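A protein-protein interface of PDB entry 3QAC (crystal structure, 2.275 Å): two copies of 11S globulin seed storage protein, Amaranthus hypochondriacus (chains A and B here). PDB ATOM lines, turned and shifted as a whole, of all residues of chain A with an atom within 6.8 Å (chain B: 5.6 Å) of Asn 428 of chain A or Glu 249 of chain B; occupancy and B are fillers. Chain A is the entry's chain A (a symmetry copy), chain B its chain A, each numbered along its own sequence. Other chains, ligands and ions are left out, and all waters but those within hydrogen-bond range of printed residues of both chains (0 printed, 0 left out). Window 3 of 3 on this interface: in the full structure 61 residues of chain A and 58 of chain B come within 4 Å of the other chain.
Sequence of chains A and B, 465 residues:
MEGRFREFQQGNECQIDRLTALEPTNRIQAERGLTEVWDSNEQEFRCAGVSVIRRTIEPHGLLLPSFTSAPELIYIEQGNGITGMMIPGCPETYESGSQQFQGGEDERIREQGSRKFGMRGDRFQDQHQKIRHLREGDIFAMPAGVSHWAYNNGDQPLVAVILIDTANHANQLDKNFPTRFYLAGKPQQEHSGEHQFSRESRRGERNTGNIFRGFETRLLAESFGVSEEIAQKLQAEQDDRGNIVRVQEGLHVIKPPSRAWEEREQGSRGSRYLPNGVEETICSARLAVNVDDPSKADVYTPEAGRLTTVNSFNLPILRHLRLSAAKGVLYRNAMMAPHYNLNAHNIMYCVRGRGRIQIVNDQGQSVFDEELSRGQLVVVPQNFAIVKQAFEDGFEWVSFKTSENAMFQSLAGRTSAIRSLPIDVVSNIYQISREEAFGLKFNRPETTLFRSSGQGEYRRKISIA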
ATOM      1  N   ILE A 423      24.778  17.633  24.339  1.00  0.00           N
ATOM      2  CA  ILE A 423      23.370  17.697  23.946  1.00  0.00           C
ATOM      3  C   ILE A 423      22.418  18.307  25.008  1.00  0.00           C
ATOM      4  O   ILE A 423      21.469  19.011  24.671  1.00  0.00           O
ATOM      5  CB  ILE A 423      22.860  16.324  23.450  1.00  0.00           C
ATOM      6  CG1 ILE A 423      21.392  16.429  23.046  1.00  0.00           C
ATOM      7  CG2 ILE A 423      23.063  15.255  24.512  1.00  0.00           C
ATOM      8  CD1 ILE A 423      21.073  15.681  21.789  1.00  0.00           C
ATOM      9  N   ASP A 424      22.687  18.045  26.283  1.00  0.00           N
ATOM     10  CA  ASP A 424      21.897  18.623  27.369  1.00  0.00           C
ATOM     11  C   ASP A 424      21.999  20.146  27.408  1.00  0.00           C
ATOM     12  O   ASP A 424      21.020  20.834  27.696  1.00  0.00           O
ATOM     13  CB  ASP A 424      22.328  18.047  28.718  1.00  0.00           C
ATOM     14  CG  ASP A 424      21.661  16.737  29.021  1.00  0.00           C
ATOM     15  OD1 ASP A 424      20.623  16.450  28.381  1.00  0.00           O
ATOM     16  OD2 ASP A 424      22.166  15.999  29.895  1.00  0.00           O
ATOM     17  N   VAL A 425      23.194  20.665  27.145  1.00  0.00           N
ATOM     18  CA  VAL A 425      23.370  22.103  27.046  1.00  0.00           C
ATOM     19  C   VAL A 425      22.520  22.614  25.894  1.00  0.00           C
ATOM     20  O   VAL A 425      21.803  23.609  26.024  1.00  0.00           O
ATOM     21  CB  VAL A 425      24.848  22.492  26.843  1.00  0.00           C
ATOM     22  CG1 VAL A 425      24.973  23.970  26.481  1.00  0.00           C
ATOM     23  CG2 VAL A 425      25.668  22.154  28.100  1.00  0.00           C
ATOM     24  N   VAL A 426      22.576  21.909  24.773  1.00  0.00           N
ATOM     25  CA  VAL A 426      21.826  22.340  23.604  1.00  0.00           C
ATOM     26  C   VAL A 426      20.318  22.396  23.893  1.00  0.00           C
ATOM     27  O   VAL A 426      19.696  23.434  23.704  1.00  0.00           O
ATOM     28  CB  VAL A 426      22.135  21.469  22.387  1.00  0.00           C
ATOM     29  CG1 VAL A 426      21.259  21.845  21.237  1.00  0.00           C
ATOM     30  CG2 VAL A 426      23.585  21.621  22.003  1.00  0.00           C
ATOM     31  N   SER A 427      19.744  21.298  24.379  1.00  0.00           N
ATOM     32  CA  SER A 427      18.305  21.262  24.631  1.00  0.00           C
ATOM     33  C   SER A 427      17.917  22.295  25.689  1.00  0.00           C
ATOM     34  O   SER A 427      16.972  23.078  25.514  1.00  0.00           O
ATOM     35  CB  SER A 427      17.848  19.853  25.030  1.00  0.00           C
ATOM     36  OG  SER A 427      18.627  19.325  26.087  1.00  0.00           O
ATOM     37  N   ASN A 428      18.675  22.319  26.777  1.00  0.00           N
ATOM     38  CA  ASN A 428      18.465  23.316  27.822  1.00  0.00           C
ATOM     39  C   ASN A 428      18.554  24.790  27.371  1.00  0.00           C
ATOM     40  O   ASN A 428      17.715  25.602  27.764  1.00  0.00           O
ATOM     41  CB  ASN A 428      19.395  23.057  29.009  1.00  0.00           C
ATOM     42  CG  ASN A 428      18.693  22.343  30.154  1.00  0.00           C
ATOM     43  OD1 ASN A 428      17.495  22.520  30.363  1.00  0.00           O
ATOM     44  ND2 ASN A 428      19.438  21.535  30.900  1.00  0.00           N
ATOM     45  N   ILE A 429      19.557  25.141  26.564  1.00  0.00           N
ATOM     46  CA  ILE A 429      19.720  26.539  26.149  1.00  0.00           C
ATOM     47  C   ILE A 429      18.724  26.921  25.078  1.00  0.00           C
ATOM     48  O   ILE A 429      18.415  28.098  24.903  1.00  0.00           O
ATOM     49  CB  ILE A 429      21.142  26.878  25.622  1.00  0.00           C
ATOM     50  CG1 ILE A 429      21.482  26.035  24.388  1.00  0.00           C
ATOM     51  CG2 ILE A 429      22.183  26.731  26.716  1.00  0.00           C
ATOM     52  CD1 ILE A 429      22.848  26.314  23.824  1.00  0.00           C
ATOM     53  N   TYR A 430      18.229  25.932  24.347  1.00  0.00           N
ATOM     54  CA  TYR A 430      17.278  26.233  23.294  1.00  0.00           C
ATOM     55  C   TYR A 430      15.861  25.859  23.701  1.00  0.00           C
ATOM     56  O   TYR A 430      14.914  26.124  22.969  1.00  0.00           O
ATOM     57  CB  TYR A 430      17.701  25.567  21.983  1.00  0.00           C
ATOM     58  CG  TYR A 430      18.991  26.146  21.452  1.00  0.00           C
ATOM     59  CD1 TYR A 430      20.109  25.338  21.248  1.00  0.00           C
ATOM     60  CD2 TYR A 430      19.111  27.516  21.201  1.00  0.00           C
ATOM     61  CE1 TYR A 430      21.300  25.863  20.771  1.00  0.00           C
ATOM     62  CE2 TYR A 430      20.299  28.059  20.728  1.00  0.00           C
ATOM     63  CZ  TYR A 430      21.398  27.225  20.513  1.00  0.00           C
ATOM     64  OH  TYR A 430      22.600  27.740  20.046  1.00  0.00           O
ATOM     65  N   GLN A 431      15.724  25.265  24.884  1.00  0.00           N
ATOM     66  CA  GLN A 431      14.414  24.858  25.391  1.00  0.00           C
ATOM     67  C   GLN A 431      13.740  23.932  24.385  1.00  0.00           C
ATOM     68  O   GLN A 431      12.673  24.233  23.852  1.00  0.00           O
ATOM     69  CB  GLN A 431      13.547  26.089  25.685  1.00  0.00           C
ATOM     70  CG  GLN A 431      14.213  27.047  26.673  1.00  0.00           C
ATOM     71  CD  GLN A 431      13.279  28.095  27.255  1.00  0.00           C
ATOM     72  OE1 GLN A 431      12.782  28.967  26.544  1.00  0.00           O
ATOM     73  NE2 GLN A 431      13.061  28.031  28.568  1.00  0.00           N
ATOM     74  N   ILE A 432      14.395  22.810  24.110  1.00  0.00           N
ATOM     75  CA  ILE A 432      13.888  21.840  23.150  1.00  0.00           C
ATOM     76  C   ILE A 432      14.190  20.432  23.667  1.00  0.00           C
ATOM     77  O   ILE A 432      14.890  20.271  24.672  1.00  0.00           O
ATOM     78  CB  ILE A 432      14.486  22.065  21.742  1.00  0.00           C
ATOM     79  CG1 ILE A 432      16.015  22.018  21.789  1.00  0.00           C
ATOM     80  CG2 ILE A 432      14.033  23.406  21.164  1.00  0.00           C
ATOM     81  CD1 ILE A 432      16.665  22.325  20.455  1.00  0.00           C
ATOM     82  N   SER A 433      13.650  19.413  23.007  1.00  0.00           N
ATOM     83  CA  SER A 433      13.807  18.051  23.499  1.00  0.00           C
ATOM     84  C   SER A 433      15.232  17.567  23.304  1.00  0.00           C
ATOM     85  O   SER A 433      16.004  18.157  22.552  1.00  0.00           O
ATOM     86  CB  SER A 433      12.837  17.085  22.810  1.00  0.00           C
ATOM     87  OG  SER A 433      13.228  16.837  21.474  1.00  0.00           O
ATOM     88  N   ALA A 437      17.169  18.537  20.019  1.00  0.00           N
ATOM     89  CA  ALA A 437      18.568  18.866  20.213  1.00  0.00           C
ATOM     90  C   ALA A 437      19.473  17.998  19.337  1.00  0.00           C
ATOM     91  O   ALA A 437      20.335  18.518  18.632  1.00  0.00           O
ATOM     92  CB  ALA A 437      18.937  18.714  21.684  1.00  0.00           C
ATOM     93  N   HIS B  60      22.779  24.813  39.513  1.00  0.00           N
ATOM     94  CA  HIS B  60      21.992  24.342  38.373  1.00  0.00           C
ATOM     95  C   HIS B  60      21.781  25.413  37.305  1.00  0.00           C
ATOM     96  O   HIS B  60      20.937  25.258  36.420  1.00  0.00           O
ATOM     97  CB  HIS B  60      20.647  23.766  38.818  1.00  0.00           C
ATOM     98  CG  HIS B  60      20.771  22.641  39.796  1.00  0.00           C
ATOM     99  ND1 HIS B  60      21.713  21.642  39.664  1.00  0.00           N
ATOM    100  CD2 HIS B  60      20.074  22.357  40.922  1.00  0.00           C
ATOM    101  CE1 HIS B  60      21.594  20.793  40.668  1.00  0.00           C
ATOM    102  NE2 HIS B  60      20.608  21.204  41.447  1.00  0.00           N
ATOM    103  N   LEU B  62      22.974  27.684  34.053  1.00  0.00           N
ATOM    104  CA  LEU B  62      23.745  27.529  32.837  1.00  0.00           C
ATOM    105  C   LEU B  62      23.997  28.877  32.156  1.00  0.00           C
ATOM    106  O   LEU B  62      23.085  29.473  31.574  1.00  0.00           O
ATOM    107  CB  LEU B  62      23.019  26.579  31.888  1.00  0.00           C
ATOM    108  CG  LEU B  62      23.623  26.355  30.509  1.00  0.00           C
ATOM    109  CD1 LEU B  62      25.015  25.777  30.634  1.00  0.00           C
ATOM    110  CD2 LEU B  62      22.742  25.418  29.753  1.00  0.00           C
ATOM    111  N   TYR B 151      28.528  26.087  33.637  1.00  0.00           N
ATOM    112  CA  TYR B 151      27.420  25.536  34.392  1.00  0.00           C
ATOM    113  C   TYR B 151      27.837  25.254  35.820  1.00  0.00           C
ATOM    114  O   TYR B 151      28.909  24.688  36.073  1.00  0.00           O
ATOM    115  CB  TYR B 151      26.904  24.270  33.724  1.00  0.00           C
ATOM    116  CG  TYR B 151      25.896  23.521  34.553  1.00  0.00           C
ATOM    117  CD1 TYR B 151      24.574  23.947  34.624  1.00  0.00           C
ATOM    118  CD2 TYR B 151      26.265  22.388  35.273  1.00  0.00           C
ATOM    119  CE1 TYR B 151      23.645  23.261  35.389  1.00  0.00           C
ATOM    120  CE2 TYR B 151      25.345  21.696  36.033  1.00  0.00           C
ATOM    121  CZ  TYR B 151      24.038  22.137  36.086  1.00  0.00           C
ATOM    122  OH  TYR B 151      23.120  21.446  36.834  1.00  0.00           O
ATOM    123  N   ARG B 241      14.642  34.328  29.860  1.00  0.00           N
ATOM    124  CA  ARG B 241      15.498  33.796  30.911  1.00  0.00           C
ATOM    125  C   ARG B 241      16.792  34.566  31.122  1.00  0.00           C
ATOM    126  O   ARG B 241      17.433  34.428  32.173  1.00  0.00           O
ATOM    127  CB  ARG B 241      15.822  32.337  30.632  1.00  0.00           C
ATOM    128  CG  ARG B 241      14.610  31.439  30.594  1.00  0.00           C
ATOM    129  CD  ARG B 241      15.026  30.066  30.128  1.00  0.00           C
ATOM    130  NE  ARG B 241      15.580  30.123  28.783  1.00  0.00           N
ATOM    131  CZ  ARG B 241      16.361  29.181  28.270  1.00  0.00           C
ATOM    132  NH1 ARG B 241      16.831  29.306  27.033  1.00  0.00           N
ATOM    133  NH2 ARG B 241      16.675  28.114  29.001  1.00  0.00           N
ATOM    134  N   VAL B 245      20.653  30.652  32.554  1.00  0.00           N
ATOM    135  CA  VAL B 245      19.387  29.949  32.635  1.00  0.00           C
ATOM    136  C   VAL B 245      19.421  28.750  33.580  1.00  0.00           C
ATOM    137  O   VAL B 245      20.480  28.185  33.852  1.00  0.00           O
ATOM    138  CB  VAL B 245      18.957  29.459  31.250  1.00  0.00           C
ATOM    139  CG1 VAL B 245      18.902  30.622  30.280  1.00  0.00           C
ATOM    140  CG2 VAL B 245      19.916  28.380  30.764  1.00  0.00           C
ATOM    141  N   ARG B 246      18.243  28.372  34.070  1.00  0.00           N
ATOM    142  CA  ARG B 246      18.104  27.265  35.010  1.00  0.00           C
ATOM    143  C   ARG B 246      17.847  25.939  34.299  1.00  0.00           C
ATOM    144  O   ARG B 246      17.050  25.869  33.369  1.00  0.00           O
ATOM    145  CB  ARG B 246      16.980  27.551  36.009  1.00  0.00           C
ATOM    146  CG  ARG B 246      16.741  26.436  37.028  1.00  0.00           C
ATOM    147  CD  ARG B 246      15.943  26.952  38.224  1.00  0.00           C
ATOM    148  NE  ARG B 246      16.564  28.139  38.822  1.00  0.00           N
ATOM    149  CZ  ARG B 246      15.948  29.309  39.010  1.00  0.00           C
ATOM    150  NH1 ARG B 246      14.673  29.469  38.661  1.00  0.00           N
ATOM    151  NH2 ARG B 246      16.612  30.323  39.561  1.00  0.00           N
ATOM    152  N   VAL B 247      18.535  24.891  34.739  1.00  0.00           N
ATOM    153  CA  VAL B 247      18.332  23.568  34.176  1.00  0.00           C
ATOM    154  C   VAL B 247      17.828  22.590  35.235  1.00  0.00           C
ATOM    155  O   VAL B 247      18.185  22.687  36.411  1.00  0.00           O
ATOM    156  CB  VAL B 247      19.625  23.039  33.537  1.00  0.00           C
ATOM    157  CG1 VAL B 247      20.555  24.199  33.216  1.00  0.00           C
ATOM    158  CG2 VAL B 247      20.318  22.054  34.455  1.00  0.00           C
ATOM    159  N   GLU B 249      16.759  19.612  36.621  1.00  0.00           N
ATOM    160  CA  GLU B 249      17.447  18.674  35.741  1.00  0.00           C
ATOM    161  C   GLU B 249      18.953  18.632  36.025  1.00  0.00           C
ATOM    162  O   GLU B 249      19.397  18.913  37.140  1.00  0.00           O
ATOM    163  CB  GLU B 249      17.190  19.048  34.277  1.00  0.00           C
ATOM    164  CG  GLU B 249      15.718  19.288  33.959  1.00  0.00           C
ATOM    165  CD  GLU B 249      15.511  20.172  32.736  1.00  0.00           C
ATOM    166  OE1 GLU B 249      14.984  19.665  31.716  1.00  0.00           O
ATOM    167  OE2 GLU B 249      15.867  21.374  32.798  1.00  0.00           O
ATOM    168  N   GLY B 250      19.730  18.273  35.008  1.00  0.00           N
ATOM    169  CA  GLY B 250      21.177  18.261  35.108  1.00  0.00           C
ATOM    170  C   GLY B 250      21.779  18.025  33.739  1.00  0.00           C
ATOM    171  O   GLY B 250      21.052  17.889  32.757  1.00  0.00           O
ATOM    172  N   LEU B 251      23.103  17.963  33.666  1.00  0.00           N
ATOM    173  CA  LEU B 251      23.789  17.763  32.387  1.00  0.00           C
ATOM    174  C   LEU B 251      24.599  16.469  32.394  1.00  0.00           C
ATOM    175  O   LEU B 251      25.327  16.188  33.352  1.00  0.00           O
ATOM    176  CB  LEU B 251      24.693  18.957  32.053  1.00  0.00           C
ATOM    177  CG  LEU B 251      24.068  20.354  32.089  1.00  0.00           C
ATOM    178  CD1 LEU B 251      23.678  20.706  33.501  1.00  0.00           C
ATOM    179  CD2 LEU B 251      25.032  21.387  31.554  1.00  0.00           C
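O of Gly 250 of chain B touches OD2 of Asp 424 of chain A (3.6 Å). Asp 424 of chain A touches Leu 251 of chain B (OD2 to CA, 3.5 Å). CG2 of Val 425 of chain A touches CD2 of Leu 251 of chain B, 3.6 Å away. ND2 of Asn 428 of chain A touches CB of Val 247 of chain B, 3.0 Å away. Leu 62 of chain B touches Ile 429 of chain A (CD2 to CG2, 3.4 Å).
Asn 428 of chain A touches just these residues of chain B: Arg 241 (3.0 Å), Val 247 (3.0 Å) and Glu 249 (3.1 Å). Printed residues of chain A within 4 Å of Arg 241 of chain B: Asn 428 (3.0 Å), Ile 429 (2.9 Å) and Gln 431 (3.2 Å). Of the printed residues of chain B, Ile 429 of chain A touches Leu 62 (3.4 Å) and Arg 241 (2.9 Å). Printed residues of chain A within 4 Å of Leu 251 of chain B: Asp 424 (3.5 Å) and Val 425 (3.6 Å). Printed residues of chain A within 4 Å of Leu 62 of chain B: Ile 429 (3.4 Å). The nearest residue of chain B that does not touch Asn 428 of chain A is Leu 62 of chain B (4.2 Å). The nearest printed residue of chain B that does not touch Gln 431 of chain A is Arg 246 of chain B (6.6 Å).
The guanidinium group (NH2) of Arg 241 of chain B lies within hydrogen-bond range of the backbone carbonyl oxygen (O) of Asn 428 of chain A, at 3.0 Å. NH1 of Arg 241 of chain B sits at hydrogen-bond distance from O of Ile 429 of chain A (2.9 Å). The side-chain amide nitrogen (NE2) of Gln 431 of chain A sits close to the guanidinium group (NE) of Arg 241 of chain B (3.3 Å). OE2 of Glu 249 of chain B sits close to OD1 of Asn 428 of chain A (3.1 Å).
No position is printed for both chains. Of the 9 pairs that touch across the chains among the printed residues, none has its exchanged pair printed and touching as well.
The backbone carbonyl oxygen (O) of His 60 of chain B is in hydrogen-bond range of the backbone NH (N) of Val 247 of chain B, 3.0 Å away. The backbone NH (N) of Leu 62 of chain B lies within hydrogen-bond range of the backbone carbonyl oxygen (O) of Val 245 of chain B (2.6 Å). The backbone carbonyl oxygen (O) of Asp 424 of chain A lies within hydrogen-bond range of the side-chain hydroxyl (OG) of Ser 427 of chain A.
Hydrophobic or aromatic side chains of chain B within 4 Å of the printed part of chain A: Leu 62, Val 247 and Leu 251.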
